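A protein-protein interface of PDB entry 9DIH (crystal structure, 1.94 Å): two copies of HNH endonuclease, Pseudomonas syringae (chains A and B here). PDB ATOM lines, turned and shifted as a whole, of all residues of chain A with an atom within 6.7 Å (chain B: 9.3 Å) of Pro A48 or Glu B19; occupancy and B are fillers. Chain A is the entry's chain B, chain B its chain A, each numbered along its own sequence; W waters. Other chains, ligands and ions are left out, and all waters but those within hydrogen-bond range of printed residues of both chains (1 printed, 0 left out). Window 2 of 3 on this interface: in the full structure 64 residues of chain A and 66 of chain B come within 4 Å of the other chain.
The side-chain carboxylate (OE1) of Glu B19 sits at hydrogen-bond distance from the backbone NH (N) of Met A49 (3.0 Å). OG1 of Thr B20 sits at hydrogen-bond distance from OH of Tyr A43 (2.9 Å). O of Asn B78 is in hydrogen-bond range of OH of Tyr A43 (3.1 Å).
OD1 of Asn B17 sits at hydrogen-bond distance from OG1 of Thr B20. The backbone NH (N) of Asn B17 sits at hydrogen-bond distance from the side-chain amide oxygen (OD1) of Asn B78 (2.9 Å). OG1 of Thr B20 sits close to OD1 of Asn B78, 3.5 Å away. O of Arg B22 lies within hydrogen-bond range of OG1 of Thr B26 (2.7 Å). The backbone NH (N) of Tyr A43 lies within hydrogen-bond range of the side-chain sulfur (SD) of Met A49, at 3.7 Å.
Glu B19 touches Tyr A43 (OE2 to CD1, 3.5 Å). Ile B23 touches Tyr A43 (CG1 to CG, 3.7 Å). Thr B80 touches Tyr A43 (CG2 to OH, 3.5 Å). Glu B19 touches Pro A48. NE of Arg B22 touches CE2 of Trp A51, 3.3 Å away. Ile B23 touches Trp A51.
Pro A48 touches one residue of chain B. Glu B19 touches three residues of chain A. Of the printed residues of chain B, Tyr A43 touches Glu B19 (3.5 Å), Thr B20 (2.9 Å), Ile B23 (3.7 Å), Asn B78 (3.1 Å) and Thr B80 (3.5 Å). Of the printed residues of chain A, Arg B22 touches Trp A51. Of the printed residues of chain B, Trp A51 touches Arg B22 (3.3 Å) and Ile B23 (3.7 Å). Of the printed residues of chain A, Thr B20 touches Tyr A43 (2.9 Å). Thr B16 touches none of the printed residues of chain A. The nearest residue of chain B that does not touch Pro A48 is Ile B23 (8.4 Å). The nearest printed residue of chain A that does not touch Asn B78 is Gly A46 (9.1 Å).
Printed residues of chain B that touch a printed residue of chain A: Glu B19, Thr B20, Arg B22, Ile B23, Asn B78 and Thr B80. Printed residues of chain A that touch a printed residue of chain B: Tyr A43, Pro A48, Met A49 and Trp A51. Hydrophobic or aromatic side chains of chain A within 4 Å of the printed part of chain B: Tyr A43, Met A49 and Trp A51.
Position printed for both chains: 54. Of the 9 pairs that touch across the chains among the printed residues, none has its exchanged pair printed and touching as well.
Water W1 lies within hydrogen-bond range of the backbone carbonyl oxygen of Asn B78 (2.7 Å), the backbone NH of Thr B80 (3.1 Å) and the side-chain hydroxyl of Tyr A43 (3.3 Å).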
ATOM      1  N   ASP A  42      -6.758 -28.590   9.438  1.00  0.00           N
ATOM      2  CA  ASP A  42      -7.640 -29.683   9.885  1.00  0.00           C
ATOM      3  C   ASP A  42      -8.696 -29.971   8.836  1.00  0.00           C
ATOM      4  O   ASP A  42      -8.947 -31.119   8.526  1.00  0.00           O
ATOM      5  CB  ASP A  42      -8.317 -29.328  11.212  1.00  0.00           C
ATOM      6  CG  ASP A  42      -7.489 -29.712  12.442  1.00  0.00           C
ATOM      7  OD1 ASP A  42      -6.459 -30.379  12.275  1.00  0.00           O
ATOM      8  OD2 ASP A  42      -7.908 -29.378  13.598  1.00  0.00           O
ATOM      9  N   TYR A  43      -9.310 -28.928   8.273  1.00  0.00           N
ATOM     10  CA  TYR A  43     -10.338 -29.142   7.283  1.00  0.00           C
ATOM     11  C   TYR A  43      -9.769 -29.815   6.046  1.00  0.00           C
ATOM     12  O   TYR A  43     -10.398 -30.728   5.476  1.00  0.00           O
ATOM     13  CB  TYR A  43     -10.965 -27.807   6.886  1.00  0.00           C
ATOM     14  CG  TYR A  43     -12.009 -27.920   5.770  1.00  0.00           C
ATOM     15  CD1 TYR A  43     -13.338 -28.254   6.058  1.00  0.00           C
ATOM     16  CD2 TYR A  43     -11.655 -27.712   4.445  1.00  0.00           C
ATOM     17  CE1 TYR A  43     -14.274 -28.315   5.061  1.00  0.00           C
ATOM     18  CE2 TYR A  43     -12.592 -27.796   3.425  1.00  0.00           C
ATOM     19  CZ  TYR A  43     -13.899 -28.099   3.741  1.00  0.00           C
ATOM     20  OH  TYR A  43     -14.833 -28.192   2.700  1.00  0.00           O
ATOM     21  N   GLY A  46      -9.716 -33.524   6.285  1.00  0.00           N
ATOM     22  CA  GLY A  46     -10.923 -34.285   6.556  1.00  0.00           C
ATOM     23  C   GLY A  46     -11.429 -34.214   7.975  1.00  0.00           C
ATOM     24  O   GLY A  46     -12.507 -34.755   8.264  1.00  0.00           O
ATOM     25  N   LYS A  47     -10.704 -33.557   8.873  1.00  0.00           N
ATOM     26  CA  LYS A  47     -11.094 -33.390  10.270  1.00  0.00           C
ATOM     27  C   LYS A  47     -12.031 -32.179  10.410  1.00  0.00           C
ATOM     28  O   LYS A  47     -12.031 -31.259   9.582  1.00  0.00           O
ATOM     29  CB  LYS A  47      -9.841 -33.186  11.124  1.00  0.00           C
ATOM     30  CG  LYS A  47     -10.072 -33.144  12.630  1.00  0.00           C
ATOM     31  CD  LYS A  47      -8.813 -32.695  13.421  1.00  0.00           C
ATOM     32  CE  LYS A  47      -7.536 -33.473  13.026  1.00  0.00           C
ATOM     33  NZ  LYS A  47      -6.379 -33.169  13.930  1.00  0.00           N
ATOM     34  N   PRO A  48     -12.883 -32.184  11.419  1.00  0.00           N
ATOM     35  CA  PRO A  48     -13.723 -31.010  11.670  1.00  0.00           C
ATOM     36  C   PRO A  48     -12.895 -29.822  12.109  1.00  0.00           C
ATOM     37  O   PRO A  48     -11.996 -29.944  12.947  1.00  0.00           O
ATOM     38  CB  PRO A  48     -14.669 -31.463  12.793  1.00  0.00           C
ATOM     39  CG  PRO A  48     -14.654 -32.949  12.742  1.00  0.00           C
ATOM     40  CD  PRO A  48     -13.287 -33.346  12.236  1.00  0.00           C
ATOM     41  N   MET A  49     -13.240 -28.656  11.573  1.00  0.00           N
ATOM     42  CA  MET A  49     -12.623 -27.413  12.029  1.00  0.00           C
ATOM     43  C   MET A  49     -13.061 -27.092  13.461  1.00  0.00           C
ATOM     44  O   MET A  49     -14.248 -26.974  13.726  1.00  0.00           O
ATOM     45  CB  MET A  49     -12.991 -26.283  11.082  1.00  0.00           C
ATOM     46  CG  MET A  49     -12.134 -26.275   9.854  1.00  0.00           C
ATOM     47  SD  MET A  49     -10.409 -26.007  10.289  1.00  0.00           S
ATOM     48  CE  MET A  49     -10.455 -24.307  10.796  1.00  0.00           C
ATOM     49  N   LYS A  50     -12.099 -26.974  14.376  1.00  0.00           N
ATOM     50  CA  LYS A  50     -12.351 -26.430  15.707  1.00  0.00           C
ATOM     51  C   LYS A  50     -11.801 -25.008  15.724  1.00  0.00           C
ATOM     52  O   LYS A  50     -10.690 -24.739  16.162  1.00  0.00           O
ATOM     53  CB  LYS A  50     -11.741 -27.307  16.782  1.00  0.00           C
ATOM     54  CG  LYS A  50     -12.381 -28.702  16.778  1.00  0.00           C
ATOM     55  CD  LYS A  50     -11.968 -29.572  17.959  1.00  0.00           C
ATOM     56  CE  LYS A  50     -12.872 -29.341  19.180  1.00  0.00           C
ATOM     57  NZ  LYS A  50     -12.476 -30.186  20.374  1.00  0.00           N
ATOM     58  N   TRP A  51     -12.622 -24.081  15.211  1.00  0.00           N
ATOM     59  CA  TRP A  51     -12.143 -22.753  14.887  1.00  0.00           C
ATOM     60  C   TRP A  51     -11.597 -22.041  16.117  1.00  0.00           C
ATOM     61  O   TRP A  51     -10.648 -21.258  16.023  1.00  0.00           O
ATOM     62  CB  TRP A  51     -13.276 -21.924  14.268  1.00  0.00           C
ATOM     63  CG  TRP A  51     -13.946 -22.500  13.031  1.00  0.00           C
ATOM     64  CD1 TRP A  51     -15.031 -23.327  13.005  1.00  0.00           C
ATOM     65  CD2 TRP A  51     -13.586 -22.275  11.675  1.00  0.00           C
ATOM     66  NE1 TRP A  51     -15.350 -23.637  11.716  1.00  0.00           N
ATOM     67  CE2 TRP A  51     -14.479 -23.002  10.878  1.00  0.00           C
ATOM     68  CE3 TRP A  51     -12.598 -21.525  11.049  1.00  0.00           C
ATOM     69  CZ2 TRP A  51     -14.417 -22.990   9.506  1.00  0.00           C
ATOM     70  CZ3 TRP A  51     -12.523 -21.553   9.673  1.00  0.00           C
ATOM     71  CH2 TRP A  51     -13.431 -22.265   8.918  1.00  0.00           C
ATOM     72  N   VAL A  54      -7.799 -23.946  17.127  1.00  0.00           N
ATOM     73  CA  VAL A  54      -6.605 -23.909  16.329  1.00  0.00           C
ATOM     74  C   VAL A  54      -6.074 -22.498  16.152  1.00  0.00           C
ATOM     75  O   VAL A  54      -5.005 -22.340  15.535  1.00  0.00           O
ATOM     76  CB  VAL A  54      -6.905 -24.556  14.962  1.00  0.00           C
ATOM     77  CG1 VAL A  54      -7.345 -26.002  15.191  1.00  0.00           C
ATOM     78  CG2 VAL A  54      -8.004 -23.747  14.230  1.00  0.00           C
ATOM     79  N   ASN B  15     -26.734 -29.757  -0.399  1.00  0.00           N
ATOM     80  CA  ASN B  15     -26.431 -28.422   0.103  1.00  0.00           C
ATOM     81  C   ASN B  15     -25.050 -28.371   0.761  1.00  0.00           C
ATOM     82  O   ASN B  15     -24.726 -29.188   1.621  1.00  0.00           O
ATOM     83  CB  ASN B  15     -27.511 -27.971   1.094  1.00  0.00           C
ATOM     84  CG  ASN B  15     -28.923 -28.185   0.570  1.00  0.00           C
ATOM     85  OD1 ASN B  15     -29.408 -27.416  -0.281  1.00  0.00           O
ATOM     86  ND2 ASN B  15     -29.595 -29.238   1.083  1.00  0.00           N
ATOM     87  N   THR B  16     -24.246 -27.407   0.350  1.00  0.00           N
ATOM     88  CA  THR B  16     -22.977 -27.117   1.004  1.00  0.00           C
ATOM     89  C   THR B  16     -23.201 -26.736   2.464  1.00  0.00           C
ATOM     90  O   THR B  16     -24.015 -25.868   2.770  1.00  0.00           O
ATOM     91  CB  THR B  16     -22.295 -25.991   0.253  1.00  0.00           C
ATOM     92  OG1 THR B  16     -22.300 -26.305  -1.150  1.00  0.00           O
ATOM     93  CG2 THR B  16     -20.825 -25.759   0.748  1.00  0.00           C
ATOM     94  N   ASN B  17     -22.494 -27.418   3.380  1.00  0.00           N
ATOM     95  CA  ASN B  17     -22.701 -27.200   4.801  1.00  0.00           C
ATOM     96  C   ASN B  17     -21.964 -25.944   5.287  1.00  0.00           C
ATOM     97  O   ASN B  17     -21.108 -25.363   4.600  1.00  0.00           O
ATOM     98  CB  ASN B  17     -22.253 -28.423   5.615  1.00  0.00           C
ATOM     99  CG  ASN B  17     -20.798 -28.669   5.479  1.00  0.00           C
ATOM    100  OD1 ASN B  17     -20.012 -27.770   5.112  1.00  0.00           O
ATOM    101  ND2 ASN B  17     -20.415 -29.861   5.719  1.00  0.00           N
ATOM    102  N   ASP B  18     -22.309 -25.530   6.523  1.00  0.00           N
ATOM    103  CA  ASP B  18     -21.865 -24.220   6.983  1.00  0.00           C
ATOM    104  C   ASP B  18     -20.342 -24.200   7.166  1.00  0.00           C
ATOM    105  O   ASP B  18     -19.680 -23.214   6.835  1.00  0.00           O
ATOM    106  CB  ASP B  18     -22.610 -23.859   8.279  1.00  0.00           C
ATOM    107  CG  ASP B  18     -22.141 -22.466   8.855  1.00  0.00           C
ATOM    108  OD1 ASP B  18     -22.237 -21.423   8.170  1.00  0.00           O
ATOM    109  OD2 ASP B  18     -21.691 -22.427  10.019  1.00  0.00           O
ATOM    110  N   GLU B  19     -19.759 -25.304   7.635  1.00  0.00           N
ATOM    111  CA  GLU B  19     -18.304 -25.344   7.764  1.00  0.00           C
ATOM    112  C   GLU B  19     -17.613 -25.061   6.463  1.00  0.00           C
ATOM    113  O   GLU B  19     -16.609 -24.332   6.404  1.00  0.00           O
ATOM    114  CB  GLU B  19     -17.898 -26.729   8.310  1.00  0.00           C
ATOM    115  CG  GLU B  19     -16.373 -26.866   8.470  1.00  0.00           C
ATOM    116  CD  GLU B  19     -15.974 -28.174   9.144  1.00  0.00           C
ATOM    117  OE1 GLU B  19     -15.925 -28.221  10.394  1.00  0.00           O
ATOM    118  OE2 GLU B  19     -15.704 -29.157   8.418  1.00  0.00           O
ATOM    119  N   THR B  20     -18.155 -25.580   5.359  1.00  0.00           N
ATOM    120  CA  THR B  20     -17.470 -25.382   4.091  1.00  0.00           C
ATOM    121  C   THR B  20     -17.632 -23.985   3.569  1.00  0.00           C
ATOM    122  O   THR B  20     -16.692 -23.414   2.967  1.00  0.00           O
ATOM    123  CB  THR B  20     -17.965 -26.362   3.079  1.00  0.00           C
ATOM    124  OG1 THR B  20     -17.606 -27.646   3.533  1.00  0.00           O
ATOM    125  CG2 THR B  20     -17.287 -26.075   1.729  1.00  0.00           C
ATOM    126  N   LYS B  21     -18.808 -23.400   3.778  1.00  0.00           N
ATOM    127  CA  LYS B  21     -19.007 -22.014   3.317  1.00  0.00           C
ATOM    128  C   LYS B  21     -18.071 -21.091   4.069  1.00  0.00           C
ATOM    129  O   LYS B  21     -17.437 -20.190   3.475  1.00  0.00           O
ATOM    130  CB  LYS B  21     -20.484 -21.642   3.503  1.00  0.00           C
ATOM    131  CG  LYS B  21     -21.376 -22.356   2.471  1.00  0.00           C
ATOM    132  CD  LYS B  21     -22.834 -22.452   2.814  1.00  0.00           C
ATOM    133  CE  LYS B  21     -23.574 -21.203   2.422  1.00  0.00           C
ATOM    134  NZ  LYS B  21     -25.078 -21.416   2.393  1.00  0.00           N
ATOM    135  N   ARG B  22     -17.920 -21.337   5.356  1.00  0.00           N
ATOM    136  CA  ARG B  22     -16.892 -20.654   6.157  1.00  0.00           C
ATOM    137  C   ARG B  22     -15.501 -20.821   5.569  1.00  0.00           C
ATOM    138  O   ARG B  22     -14.730 -19.860   5.479  1.00  0.00           O
ATOM    139  CB  ARG B  22     -16.979 -21.234   7.559  1.00  0.00           C
ATOM    140  CG  ARG B  22     -16.680 -20.296   8.610  1.00  0.00           C
ATOM    141  CD  ARG B  22     -17.182 -20.850   9.919  1.00  0.00           C
ATOM    142  NE  ARG B  22     -16.376 -20.255  10.976  1.00  0.00           N
ATOM    143  CZ  ARG B  22     -16.762 -20.154  12.227  1.00  0.00           C
ATOM    144  NH1 ARG B  22     -17.929 -20.637  12.613  1.00  0.00           N
ATOM    145  NH2 ARG B  22     -15.965 -19.538  13.097  1.00  0.00           N
ATOM    146  N   ILE B  23     -15.162 -22.034   5.138  1.00  0.00           N
ATOM    147  CA  ILE B  23     -13.856 -22.239   4.536  1.00  0.00           C
ATOM    148  C   ILE B  23     -13.730 -21.434   3.258  1.00  0.00           C
ATOM    149  O   ILE B  23     -12.673 -20.832   2.992  1.00  0.00           O
ATOM    150  CB  ILE B  23     -13.588 -23.731   4.276  1.00  0.00           C
ATOM    151  CG1 ILE B  23     -13.266 -24.396   5.610  1.00  0.00           C
ATOM    152  CG2 ILE B  23     -12.519 -23.850   3.219  1.00  0.00           C
ATOM    153  CD1 ILE B  23     -11.846 -24.100   6.059  1.00  0.00           C
ATOM    154  N   VAL B  24     -14.803 -21.402   2.428  1.00  0.00           N
ATOM    155  CA  VAL B  24     -14.742 -20.667   1.180  1.00  0.00           C
ATOM    156  C   VAL B  24     -14.567 -19.177   1.439  1.00  0.00           C
ATOM    157  O   VAL B  24     -13.843 -18.477   0.699  1.00  0.00           O
ATOM    158  CB  VAL B  24     -15.971 -20.956   0.343  1.00  0.00           C
ATOM    159  CG1 VAL B  24     -16.021 -20.000  -0.859  1.00  0.00           C
ATOM    160  CG2 VAL B  24     -15.952 -22.403  -0.092  1.00  0.00           C
ATOM    161  N   TRP B  25     -15.257 -18.648   2.426  1.00  0.00           N
ATOM    162  CA  TRP B  25     -15.086 -17.228   2.744  1.00  0.00           C
ATOM    163  C   TRP B  25     -13.694 -16.972   3.272  1.00  0.00           C
ATOM    164  O   TRP B  25     -13.014 -16.063   2.805  1.00  0.00           O
ATOM    165  CB  TRP B  25     -16.131 -16.793   3.806  1.00  0.00           C
ATOM    166  CG  TRP B  25     -17.468 -16.441   3.210  1.00  0.00           C
ATOM    167  CD1 TRP B  25     -18.537 -17.305   2.973  1.00  0.00           C
ATOM    168  CD2 TRP B  25     -17.895 -15.166   2.779  1.00  0.00           C
ATOM    169  NE1 TRP B  25     -19.558 -16.620   2.413  1.00  0.00           N
ATOM    170  CE2 TRP B  25     -19.213 -15.297   2.306  1.00  0.00           C
ATOM    171  CE3 TRP B  25     -17.315 -13.895   2.793  1.00  0.00           C
ATOM    172  CZ2 TRP B  25     -19.946 -14.221   1.834  1.00  0.00           C
ATOM    173  CZ3 TRP B  25     -18.058 -12.812   2.323  1.00  0.00           C
ATOM    174  CH2 TRP B  25     -19.352 -12.984   1.823  1.00  0.00           C
ATOM    175  N   THR B  26     -13.206 -17.837   4.144  1.00  0.00           N
ATOM    176  CA  THR B  26     -11.853 -17.677   4.666  1.00  0.00           C
ATOM    177  C   THR B  26     -10.806 -17.680   3.577  1.00  0.00           C
ATOM    178  O   THR B  26      -9.972 -16.772   3.514  1.00  0.00           O
ATOM    179  CB  THR B  26     -11.561 -18.773   5.645  1.00  0.00           C
ATOM    180  OG1 THR B  26     -12.536 -18.741   6.654  1.00  0.00           O
ATOM    181  CG2 THR B  26     -10.144 -18.497   6.238  1.00  0.00           C
ATOM    182  N   GLN B  27     -10.803 -18.694   2.714  1.00  0.00           N
ATOM    183  CA  GLN B  27      -9.653 -18.844   1.792  1.00  0.00           C
ATOM    184  C   GLN B  27      -9.635 -17.845   0.686  1.00  0.00           C
ATOM    185  O   GLN B  27      -8.593 -17.670   0.015  1.00  0.00           O
ATOM    186  CB  GLN B  27      -9.622 -20.239   1.169  1.00  0.00           C
ATOM    187  CG  GLN B  27     -10.846 -20.587   0.370  1.00  0.00           C
ATOM    188  CD  GLN B  27     -10.819 -22.036  -0.149  1.00  0.00           C
ATOM    189  OE1 GLN B  27     -10.148 -22.901   0.427  1.00  0.00           O
ATOM    190  NE2 GLN B  27     -11.507 -22.275  -1.259  1.00  0.00           N
ATOM    191  N   VAL B  54     -21.687 -18.336  -2.384  1.00  0.00           N
ATOM    192  CA  VAL B  54     -20.834 -19.493  -2.647  1.00  0.00           C
ATOM    193  C   VAL B  54     -21.341 -20.223  -3.886  1.00  0.00           C
ATOM    194  O   VAL B  54     -22.424 -20.817  -3.862  1.00  0.00           O
ATOM    195  CB  VAL B  54     -20.836 -20.426  -1.419  1.00  0.00           C
ATOM    196  CG1 VAL B  54     -20.003 -21.678  -1.694  1.00  0.00           C
ATOM    197  CG2 VAL B  54     -20.325 -19.677  -0.227  1.00  0.00           C
ATOM    198  N   ASN B  78     -19.162 -30.556  -0.848  1.00  0.00           N
ATOM    199  CA  ASN B  78     -18.296 -29.735  -0.007  1.00  0.00           C
ATOM    200  C   ASN B  78     -16.853 -29.803  -0.477  1.00  0.00           C
ATOM    201  O   ASN B  78     -15.907 -29.827   0.330  1.00  0.00           O
ATOM    202  CB  ASN B  78     -18.407 -30.157   1.459  1.00  0.00           C
ATOM    203  CG  ASN B  78     -19.866 -30.018   1.989  1.00  0.00           C
ATOM    204  OD1 ASN B  78     -20.466 -28.938   1.987  1.00  0.00           O
ATOM    205  ND2 ASN B  78     -20.422 -31.106   2.422  1.00  0.00           N
ATOM    206  N   THR B  80     -14.194 -27.764  -2.026  1.00  0.00           N
ATOM    207  CA  THR B  80     -13.913 -26.357  -2.312  1.00  0.00           C
ATOM    208  C   THR B  80     -13.170 -26.154  -3.635  1.00  0.00           C
ATOM    209  O   THR B  80     -13.007 -25.004  -4.073  1.00  0.00           O
ATOM    210  CB  THR B  80     -13.138 -25.714  -1.179  1.00  0.00           C
ATOM    211  OG1 THR B  80     -11.803 -26.185  -1.194  1.00  0.00           O
ATOM    212  CG2 THR B  80     -13.832 -26.000   0.175  1.00  0.00           C
ATOM    213  N   LEU B  83     -16.024 -24.843  -5.572  1.00  0.00           N
ATOM    214  CA  LEU B  83     -16.799 -23.749  -5.010  1.00  0.00           C
ATOM    215  C   LEU B  83     -15.993 -22.459  -5.031  1.00  0.00           C
ATOM    216  O   LEU B  83     -14.879 -22.407  -4.507  1.00  0.00           O
ATOM    217  CB  LEU B  83     -17.269 -24.061  -3.582  1.00  0.00           C
ATOM    218  CG  LEU B  83     -18.015 -25.385  -3.423  1.00  0.00           C
ATOM    219  CD1 LEU B  83     -18.167 -25.809  -1.988  1.00  0.00           C
ATOM    220  CD2 LEU B  83     -19.364 -25.268  -4.073  1.00  0.00           C
HETATM  221  O   HOH W   1     -13.218 -29.635   0.180  1.00  0.00           O
